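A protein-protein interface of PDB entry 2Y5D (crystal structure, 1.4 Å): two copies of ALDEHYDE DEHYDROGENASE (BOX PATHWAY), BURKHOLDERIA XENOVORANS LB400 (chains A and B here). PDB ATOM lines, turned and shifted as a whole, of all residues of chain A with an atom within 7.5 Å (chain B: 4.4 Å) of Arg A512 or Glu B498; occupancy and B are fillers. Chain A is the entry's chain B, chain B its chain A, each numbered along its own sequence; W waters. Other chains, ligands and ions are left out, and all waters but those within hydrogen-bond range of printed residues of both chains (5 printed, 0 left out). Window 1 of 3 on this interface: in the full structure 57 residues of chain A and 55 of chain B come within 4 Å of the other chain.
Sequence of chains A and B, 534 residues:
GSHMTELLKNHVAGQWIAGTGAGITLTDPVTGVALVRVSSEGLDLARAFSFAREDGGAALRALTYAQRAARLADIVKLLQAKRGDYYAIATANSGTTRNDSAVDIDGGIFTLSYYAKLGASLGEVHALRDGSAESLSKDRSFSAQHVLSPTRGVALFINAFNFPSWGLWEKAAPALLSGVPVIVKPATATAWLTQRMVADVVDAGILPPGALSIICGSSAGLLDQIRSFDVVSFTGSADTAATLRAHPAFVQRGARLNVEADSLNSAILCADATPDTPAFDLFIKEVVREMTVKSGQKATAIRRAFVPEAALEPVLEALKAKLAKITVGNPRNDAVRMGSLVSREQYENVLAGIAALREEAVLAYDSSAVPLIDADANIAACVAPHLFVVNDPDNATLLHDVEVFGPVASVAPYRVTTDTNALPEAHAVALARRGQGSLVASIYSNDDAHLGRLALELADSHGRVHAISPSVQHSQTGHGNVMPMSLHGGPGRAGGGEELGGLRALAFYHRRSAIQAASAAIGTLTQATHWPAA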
ATOM      1  N   ASP A 130      31.891   9.316  -8.844  1.00  0.00           N
ATOM      2  CA  ASP A 130      30.624   8.644  -8.833  1.00  0.00           C
ATOM      3  C   ASP A 130      29.867   8.972 -10.123  1.00  0.00           C
ATOM      4  O   ASP A 130      29.299  10.056 -10.296  1.00  0.00           O
ATOM      5  CB  ASP A 130      29.833   9.154  -7.609  1.00  0.00           C
ATOM      6  CG  ASP A 130      28.367   8.712  -7.626  1.00  0.00           C
ATOM      7  OD1 ASP A 130      27.807   8.023  -8.414  1.00  0.00           O
ATOM      8  OD2 ASP A 130      27.593   9.357  -6.869  1.00  0.00           O
ATOM      9  N   HIS A 146      29.544  14.009  -9.893  1.00  0.00           N
ATOM     10  CA  HIS A 146      29.507  13.640  -8.462  1.00  0.00           C
ATOM     11  C   HIS A 146      30.799  12.976  -8.040  1.00  0.00           C
ATOM     12  O   HIS A 146      31.472  12.277  -8.867  1.00  0.00           O
ATOM     13  CB  HIS A 146      28.351  12.680  -8.228  1.00  0.00           C
ATOM     14  CG  HIS A 146      27.007  13.312  -8.408  1.00  0.00           C
ATOM     15  ND1 HIS A 146      26.398  13.549  -9.626  1.00  0.00           N
ATOM     16  CD2 HIS A 146      26.135  13.760  -7.453  1.00  0.00           C
ATOM     17  CE1 HIS A 146      25.217  14.158  -9.443  1.00  0.00           C
ATOM     18  NE2 HIS A 146      25.014  14.229  -8.114  1.00  0.00           N
ATOM     19  N   VAL A 147      31.184  13.194  -6.787  1.00  0.00           N
ATOM     20  CA  VAL A 147      32.429  12.596  -6.255  1.00  0.00           C
ATOM     21  C   VAL A 147      32.098  12.046  -4.855  1.00  0.00           C
ATOM     22  O   VAL A 147      31.102  12.434  -4.223  1.00  0.00           O
ATOM     23  CB  VAL A 147      33.568  13.612  -6.085  1.00  0.00           C
ATOM     24  CG1 VAL A 147      33.990  14.141  -7.537  1.00  0.00           C
ATOM     25  CG2 VAL A 147      33.230  14.793  -5.168  1.00  0.00           C
ATOM     26  N   LEU A 148      32.975  11.164  -4.387  1.00  0.00           N
ATOM     27  CA  LEU A 148      32.932  10.583  -3.071  1.00  0.00           C
ATOM     28  C   LEU A 148      34.197  10.914  -2.333  1.00  0.00           C
ATOM     29  O   LEU A 148      35.280  10.633  -2.847  1.00  0.00           O
ATOM     30  CB  LEU A 148      32.803   9.024  -3.128  1.00  0.00           C
ATOM     31  CG  LEU A 148      31.589   8.495  -3.831  1.00  0.00           C
ATOM     32  CD1 LEU A 148      31.787   6.956  -3.906  1.00  0.00           C
ATOM     33  CD2 LEU A 148      30.364   8.757  -3.054  1.00  0.00           C
ATOM     34  N   SER A 149      34.069  11.483  -1.154  1.00  0.00           N
ATOM     35  CA  SER A 149      35.216  11.873  -0.323  1.00  0.00           C
ATOM     36  C   SER A 149      35.157  11.127   1.002  1.00  0.00           C
ATOM     37  O   SER A 149      34.065  11.018   1.592  1.00  0.00           O
ATOM     38  CB  SER A 149      35.177  13.377  -0.033  1.00  0.00           C
ATOM     39  OG  SER A 149      35.136  14.109  -1.208  1.00  0.00           O
ATOM     40  N   ARG A 256      25.727   8.249  10.962  1.00  0.00           N
ATOM     41  CA  ARG A 256      25.201   7.101  10.238  1.00  0.00           C
ATOM     42  C   ARG A 256      25.246   5.894  11.085  1.00  0.00           C
ATOM     43  O   ARG A 256      26.197   5.650  11.917  1.00  0.00           O
ATOM     44  CB  ARG A 256      26.052   6.781   8.989  1.00  0.00           C
ATOM     45  CG  ARG A 256      25.917   7.878   8.076  1.00  0.00           C
ATOM     46  CD  ARG A 256      26.680   7.444   6.714  1.00  0.00           C
ATOM     47  NE  ARG A 256      26.411   8.469   5.670  1.00  0.00           N
ATOM     48  CZ  ARG A 256      27.148   8.675   4.575  1.00  0.00           C
ATOM     49  NH1 ARG A 256      28.249   7.977   4.447  1.00  0.00           N
ATOM     50  NH2 ARG A 256      26.845   9.628   3.763  1.00  0.00           N
ATOM     51  N   ARG A 504      30.246  -1.528  -3.321  1.00  0.00           N
ATOM     52  CA  ARG A 504      29.056  -0.898  -2.666  1.00  0.00           C
ATOM     53  C   ARG A 504      29.333  -0.564  -1.235  1.00  0.00           C
ATOM     54  O   ARG A 504      28.760   0.411  -0.747  1.00  0.00           O
ATOM     55  CB  ARG A 504      27.838  -1.790  -2.777  1.00  0.00           C
ATOM     56  CG  ARG A 504      27.400  -2.052  -4.254  1.00  0.00           C
ATOM     57  CD  ARG A 504      26.370  -3.223  -4.327  1.00  0.00           C
ATOM     58  NE  ARG A 504      26.062  -3.451  -5.769  1.00  0.00           N
ATOM     59  CZ  ARG A 504      26.844  -4.184  -6.532  1.00  0.00           C
ATOM     60  NH1 ARG A 504      27.932  -4.813  -6.055  1.00  0.00           N
ATOM     61  NH2 ARG A 504      26.405  -4.413  -7.808  1.00  0.00           N
ATOM     62  N   LEU A 506      31.786   0.906   0.014  1.00  0.00           N
ATOM     63  CA  LEU A 506      32.528   2.194   0.196  1.00  0.00           C
ATOM     64  C   LEU A 506      31.606   3.322   0.457  1.00  0.00           C
ATOM     65  O   LEU A 506      32.034   4.277   1.161  1.00  0.00           O
ATOM     66  CB  LEU A 506      33.375   2.491  -1.098  1.00  0.00           C
ATOM     67  CG  LEU A 506      34.316   1.405  -1.417  1.00  0.00           C
ATOM     68  CD1 LEU A 506      35.002   1.761  -2.792  1.00  0.00           C
ATOM     69  CD2 LEU A 506      35.409   1.161  -0.354  1.00  0.00           C
ATOM     70  N   ALA A 507      30.379   3.320   0.014  1.00  0.00           N
ATOM     71  CA  ALA A 507      29.553   4.521   0.155  1.00  0.00           C
ATOM     72  C   ALA A 507      29.277   4.896   1.632  1.00  0.00           C
ATOM     73  O   ALA A 507      29.251   6.094   1.943  1.00  0.00           O
ATOM     74  CB  ALA A 507      28.179   4.321  -0.620  1.00  0.00           C
ATOM     75  N   PHE A 508      29.134   3.913   2.487  1.00  0.00           N
ATOM     76  CA  PHE A 508      28.834   4.139   3.943  1.00  0.00           C
ATOM     77  C   PHE A 508      29.932   4.965   4.558  1.00  0.00           C
ATOM     78  O   PHE A 508      29.642   5.709   5.534  1.00  0.00           O
ATOM     79  CB  PHE A 508      28.677   2.779   4.584  1.00  0.00           C
ATOM     80  CG  PHE A 508      28.361   2.807   6.058  1.00  0.00           C
ATOM     81  CD1 PHE A 508      27.071   3.161   6.437  1.00  0.00           C
ATOM     82  CD2 PHE A 508      29.344   2.367   6.893  1.00  0.00           C
ATOM     83  CE1 PHE A 508      26.736   3.150   7.803  1.00  0.00           C
ATOM     84  CE2 PHE A 508      28.986   2.316   8.258  1.00  0.00           C
ATOM     85  CZ  PHE A 508      27.679   2.719   8.688  1.00  0.00           C
ATOM     86  N   HIS A 510      31.858   7.248   2.878  1.00  0.00           N
ATOM     87  CA  HIS A 510      32.145   8.496   2.113  1.00  0.00           C
ATOM     88  C   HIS A 510      31.024   9.457   2.166  1.00  0.00           C
ATOM     89  O   HIS A 510      29.839   9.084   2.484  1.00  0.00           O
ATOM     90  CB  HIS A 510      32.389   8.123   0.626  1.00  0.00           C
ATOM     91  CG  HIS A 510      33.712   7.442   0.334  1.00  0.00           C
ATOM     92  ND1 HIS A 510      34.012   6.123   0.570  1.00  0.00           N
ATOM     93  CD2 HIS A 510      34.846   7.958  -0.211  1.00  0.00           C
ATOM     94  CE1 HIS A 510      35.283   5.845   0.214  1.00  0.00           C
ATOM     95  NE2 HIS A 510      35.814   6.970  -0.223  1.00  0.00           N
ATOM     96  N   ARG A 511      31.287  10.665   1.808  1.00  0.00           N
ATOM     97  CA  ARG A 511      30.339  11.706   1.599  1.00  0.00           C
ATOM     98  C   ARG A 511      30.189  11.955   0.115  1.00  0.00           C
ATOM     99  O   ARG A 511      31.251  12.205  -0.553  1.00  0.00           O
ATOM    100  CB  ARG A 511      30.942  13.011   2.219  1.00  0.00           C
ATOM    101  CG  ARG A 511      31.179  12.884   3.687  1.00  0.00           C
ATOM    102  CD  ARG A 511      29.567  13.018   4.041  1.00  0.00           C
ATOM    103  NE  ARG A 511      29.562  12.414   5.260  1.00  0.00           N
ATOM    104  CZ  ARG A 511      28.665  12.007   6.134  1.00  0.00           C
ATOM    105  NH1 ARG A 511      29.281  11.408   7.076  1.00  0.00           N
ATOM    106  NH2 ARG A 511      27.314  11.975   6.060  1.00  0.00           N
ATOM    107  N   ARG A 512      29.005  11.873  -0.445  1.00  0.00           N
ATOM    108  CA  ARG A 512      28.788  12.138  -1.886  1.00  0.00           C
ATOM    109  C   ARG A 512      28.545  13.626  -2.078  1.00  0.00           C
ATOM    110  O   ARG A 512      27.801  14.244  -1.265  1.00  0.00           O
ATOM    111  CB  ARG A 512      27.657  11.302  -2.350  1.00  0.00           C
ATOM    112  CG  ARG A 512      27.428  11.408  -3.857  1.00  0.00           C
ATOM    113  CD  ARG A 512      26.148  10.502  -4.221  1.00  0.00           C
ATOM    114  NE  ARG A 512      26.595   9.145  -4.215  1.00  0.00           N
ATOM    115  CZ  ARG A 512      26.350   8.234  -3.262  1.00  0.00           C
ATOM    116  NH1 ARG A 512      25.625   8.591  -2.163  1.00  0.00           N
ATOM    117  NH2 ARG A 512      26.871   6.973  -3.295  1.00  0.00           N
ATOM    118  N   SER A 513      29.109  14.233  -3.122  1.00  0.00           N
ATOM    119  CA  SER A 513      28.832  15.642  -3.422  1.00  0.00           C
ATOM    120  C   SER A 513      28.638  15.812  -4.893  1.00  0.00           C
ATOM    121  O   SER A 513      29.384  15.167  -5.674  1.00  0.00           O
ATOM    122  CB  SER A 513      30.031  16.471  -2.958  1.00  0.00           C
ATOM    123  OG  SER A 513      29.799  17.950  -3.121  1.00  0.00           O
ATOM    124  N   ALA A 514      27.749  16.683  -5.354  1.00  0.00           N
ATOM    125  CA  ALA A 514      27.615  17.080  -6.757  1.00  0.00           C
ATOM    126  C   ALA A 514      28.432  18.321  -6.932  1.00  0.00           C
ATOM    127  O   ALA A 514      28.214  19.348  -6.311  1.00  0.00           O
ATOM    128  CB  ALA A 514      26.112  17.435  -7.002  1.00  0.00           C
ATOM    129  N   ILE A 515      29.396  18.251  -7.867  1.00  0.00           N
ATOM    130  CA  ILE A 515      30.153  19.478  -8.194  1.00  0.00           C
ATOM    131  C   ILE A 515      29.679  19.974  -9.511  1.00  0.00           C
ATOM    132  O   ILE A 515      29.672  19.281 -10.545  1.00  0.00           O
ATOM    133  CB  ILE A 515      31.668  19.111  -8.352  1.00  0.00           C
ATOM    134  CG1 ILE A 515      32.193  18.303  -7.214  1.00  0.00           C
ATOM    135  CG2 ILE A 515      32.434  20.442  -8.587  1.00  0.00           C
ATOM    136  CD1 ILE A 515      32.037  18.822  -5.921  1.00  0.00           C
ATOM    137  N   ASN B 258      14.676  10.221   5.477  1.00  0.00           N
ATOM    138  CA  ASN B 258      15.608  11.218   4.849  1.00  0.00           C
ATOM    139  C   ASN B 258      15.291  12.486   5.537  1.00  0.00           C
ATOM    140  O   ASN B 258      14.082  12.870   5.525  1.00  0.00           O
ATOM    141  CB  ASN B 258      15.446  11.266   3.360  1.00  0.00           C
ATOM    142  CG  ASN B 258      16.555  12.112   2.710  1.00  0.00           C
ATOM    143  OD1 ASN B 258      16.332  13.302   2.311  1.00  0.00           O
ATOM    144  ND2 ASN B 258      17.690  11.531   2.650  1.00  0.00           N
ATOM    145  N   GLU B 260      16.143  16.696   5.343  1.00  0.00           N
ATOM    146  CA  GLU B 260      16.775  17.888   4.711  1.00  0.00           C
ATOM    147  C   GLU B 260      16.494  18.950   5.671  1.00  0.00           C
ATOM    148  O   GLU B 260      15.279  19.344   5.891  1.00  0.00           O
ATOM    149  CB  GLU B 260      16.146  18.080   3.291  1.00  0.00           C
ATOM    150  CG  GLU B 260      16.382  16.812   2.318  1.00  0.00           C
ATOM    151  CD  GLU B 260      17.655  16.865   1.477  1.00  0.00           C
ATOM    152  OE1 GLU B 260      18.199  18.002   1.308  1.00  0.00           O
ATOM    153  OE2 GLU B 260      18.045  15.748   0.988  1.00  0.00           O
ATOM    154  N   GLY B 463      26.965  18.977   0.377  1.00  0.00           N
ATOM    155  CA  GLY B 463      26.366  18.012  -0.637  1.00  0.00           C
ATOM    156  C   GLY B 463      26.489  18.483  -2.061  1.00  0.00           C
ATOM    157  O   GLY B 463      26.333  17.687  -2.934  1.00  0.00           O
ATOM    158  N   LEU B 487      22.723  15.773  -6.922  1.00  0.00           N
ATOM    159  CA  LEU B 487      22.362  15.491  -5.544  1.00  0.00           C
ATOM    160  C   LEU B 487      21.947  16.699  -4.825  1.00  0.00           C
ATOM    161  O   LEU B 487      22.515  17.797  -4.921  1.00  0.00           O
ATOM    162  CB  LEU B 487      23.619  14.949  -4.879  1.00  0.00           C
ATOM    163  CG  LEU B 487      23.464  14.330  -3.484  1.00  0.00           C
ATOM    164  CD1 LEU B 487      22.768  12.930  -3.848  1.00  0.00           C
ATOM    165  CD2 LEU B 487      24.868  14.094  -2.777  1.00  0.00           C
ATOM    166  N   HIS B 488      20.930  16.512  -3.972  1.00  0.00           N
ATOM    167  CA  HIS B 488      20.413  17.501  -3.037  1.00  0.00           C
ATOM    168  C   HIS B 488      20.388  17.036  -1.600  1.00  0.00           C
ATOM    169  O   HIS B 488      19.674  16.054  -1.314  1.00  0.00           O
ATOM    170  CB  HIS B 488      19.044  17.999  -3.488  1.00  0.00           C
ATOM    171  CG  HIS B 488      18.466  19.047  -2.599  1.00  0.00           C
ATOM    172  ND1 HIS B 488      19.066  20.299  -2.392  1.00  0.00           N
ATOM    173  CD2 HIS B 488      17.360  19.021  -1.791  1.00  0.00           C
ATOM    174  CE1 HIS B 488      18.355  20.982  -1.505  1.00  0.00           C
ATOM    175  NE2 HIS B 488      17.299  20.222  -1.163  1.00  0.00           N
ATOM    176  N   GLY B 497      21.069  13.754   4.684  1.00  0.00           N
ATOM    177  CA  GLY B 497      20.174  13.198   3.638  1.00  0.00           C
ATOM    178  C   GLY B 497      20.685  13.315   2.239  1.00  0.00           C
ATOM    179  O   GLY B 497      21.677  14.070   1.976  1.00  0.00           O
ATOM    180  N   GLU B 498      20.003  12.627   1.334  1.00  0.00           N
ATOM    181  CA  GLU B 498      20.293  12.724  -0.119  1.00  0.00           C
ATOM    182  C   GLU B 498      18.984  12.512  -0.853  1.00  0.00           C
ATOM    183  O   GLU B 498      18.238  11.543  -0.506  1.00  0.00           O
ATOM    184  CB  GLU B 498      21.265  11.578  -0.487  1.00  0.00           C
ATOM    185  CG  GLU B 498      22.614  11.743   0.191  1.00  0.00           C
ATOM    186  CD  GLU B 498      23.734  10.916  -0.389  1.00  0.00           C
ATOM    187  OE1 GLU B 498      23.680  10.302  -1.505  1.00  0.00           O
ATOM    188  OE2 GLU B 498      24.797  10.942   0.298  1.00  0.00           O
ATOM    189  N   GLU B 499      18.756  13.362  -1.788  1.00  0.00           N
ATOM    190  CA  GLU B 499      17.603  13.364  -2.681  1.00  0.00           C
ATOM    191  C   GLU B 499      18.112  13.656  -4.082  1.00  0.00           C
ATOM    192  O   GLU B 499      19.222  14.137  -4.246  1.00  0.00           O
ATOM    193  CB  GLU B 499      16.606  14.612  -2.352  1.00  0.00           C
ATOM    194  CG  GLU B 499      16.143  14.664  -1.062  1.00  0.00           C
ATOM    195  CD  GLU B 499      15.010  15.554  -0.956  1.00  0.00           C
ATOM    196  OE1 GLU B 499      15.047  16.795  -1.049  1.00  0.00           O
ATOM    197  OE2 GLU B 499      14.034  15.013  -0.764  1.00  0.00           O
ATOM    198  N   ARG B 504      20.006   8.327  -8.977  1.00  0.00           N
ATOM    199  CA  ARG B 504      20.418   8.050  -7.601  1.00  0.00           C
ATOM    200  C   ARG B 504      19.211   8.138  -6.674  1.00  0.00           C
ATOM    201  O   ARG B 504      19.173   7.316  -5.690  1.00  0.00           O
ATOM    202  CB  ARG B 504      21.474   9.046  -7.100  1.00  0.00           C
ATOM    203  CG  ARG B 504      22.811   8.870  -7.878  1.00  0.00           C
ATOM    204  CD  ARG B 504      23.747  10.026  -7.544  1.00  0.00           C
ATOM    205  NE  ARG B 504      25.000   9.910  -8.386  1.00  0.00           N
ATOM    206  CZ  ARG B 504      24.991  10.371  -9.619  1.00  0.00           C
ATOM    207  NH1 ARG B 504      23.923  10.924 -10.230  1.00  0.00           N
ATOM    208  NH2 ARG B 504      26.187  10.218 -10.327  1.00  0.00           N
HETATM  209  O   HOH W   1      27.152  10.324   1.060  1.00  0.00           O
HETATM  210  O   HOH W   2      24.236  10.579   3.068  1.00  0.00           O
HETATM  211  O   HOH W   3      26.001  13.387   0.734  1.00  0.00           O
HETATM  212  O   HOH W   4      28.359  12.163 -11.735  1.00  0.00           O
HETATM  213  O   HOH W   5      25.448   7.023  -6.510  1.00  0.00           O
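Leu B487 touches Arg A512. N of Leu B487 touches CB of Ala A514, 3.8 Å away.
Position printed for both chains: 504. Of the 8 pairs that touch across the chains among the printed residues, none has its exchanged pair printed and touching as well.
N of Val A147 sits at hydrogen-bond distance from O of Ser A513, at 2.9 Å. OD2 of Asp A130 is in salt-bridge range of NE of Arg A512 (2.8 Å). N of Glu B498 sits close to ND2 of Asn B258 (2.9 Å). The backbone NH (N) of Asp A130 sits at hydrogen-bond distance from the backbone carbonyl oxygen (O) of His A146.
OE1 of Glu B498 is in salt-bridge range of NH1 of Arg A512. The backbone carbonyl oxygen of Gly B463 sits close to the side-chain hydroxyl of Ser A513, 3.5 Å away. N of Leu B487 is in hydrogen-bond range of NE2 of His A146 (3.0 Å). The backbone carbonyl oxygen (O) of Gly B463 lies within hydrogen-bond range of the backbone NH (N) of Ala A514 (3.0 Å). The guanidinium group of Arg B504 sits at hydrogen-bond distance from a ring nitrogen (ND1) of His A146, 3.4 Å away. The side-chain carboxylate (OD2) of Asp A130 lies within salt-bridge range of the guanidinium group (NE) of Arg B504 (3.1 Å).
Of the 16 printed residues of chain A, 5 touch a printed residue of chain B. Hydrophobic or aromatic side chains of chain B within 4 Å of the printed part of chain A: Leu B487. Among the printed residues, 8 pairs touch across the chains. Among the printed residues, Asp or Glu carboxylates within 4 Å of a Lys or Arg side-chain nitrogen of the other chain: Asp A130 with Arg B504 (3.1 Å) and Arg A512 with Glu B498 (2.7 Å).
Arg A512 touches just these residues of chain B: Leu B487 (3.3 Å) and Glu B498 (2.7 Å). Printed residues of chain A within 4 Å of Glu B498: Arg A512 (2.7 Å). Of the printed residues of chain A, Arg B504 touches Asp A130 and His A146. Of the printed residues of chain B, His A146 touches Leu B487 (3.0 Å) and Arg B504 (3.4 Å). Of the printed residues of chain B, Asp A130 touches Arg B504 (3.1 Å). The nearest residue of chain B that does not touch Arg A512 is Gly B463 (4.1 Å).
Water W1 lies within hydrogen-bond range of the side-chain carboxylate (OE2) of Glu B498 (2.6 Å), the guanidinium group (NH2) of Arg A256 (2.8 Å), the backbone NH (N) of Arg A512 (2.8 Å) and the backbone carbonyl oxygen (O) of His A510 (3.3 Å). Water W4 lies within hydrogen-bond range of the backbone carbonyl oxygen (O) of Asp A130 (2.7 Å), the backbone NH (N) of His A146 (2.9 Å) and the guanidinium group (NH2) of Arg B504 (3.2 Å). Water W3 bridges the side-chain carboxylate of Glu B498 and the backbone carbonyl oxygen of Arg A512. Water W2 lies within hydrogen-bond range of OE2 of Glu B498 (2.8 Å) and NH2 of Arg A256 (2.9 Å). Water W5 lies within hydrogen-bond range of the side-chain carboxylate of Asp A130, the guanidinium group of Arg A512 and the guanidinium group of Arg B504.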
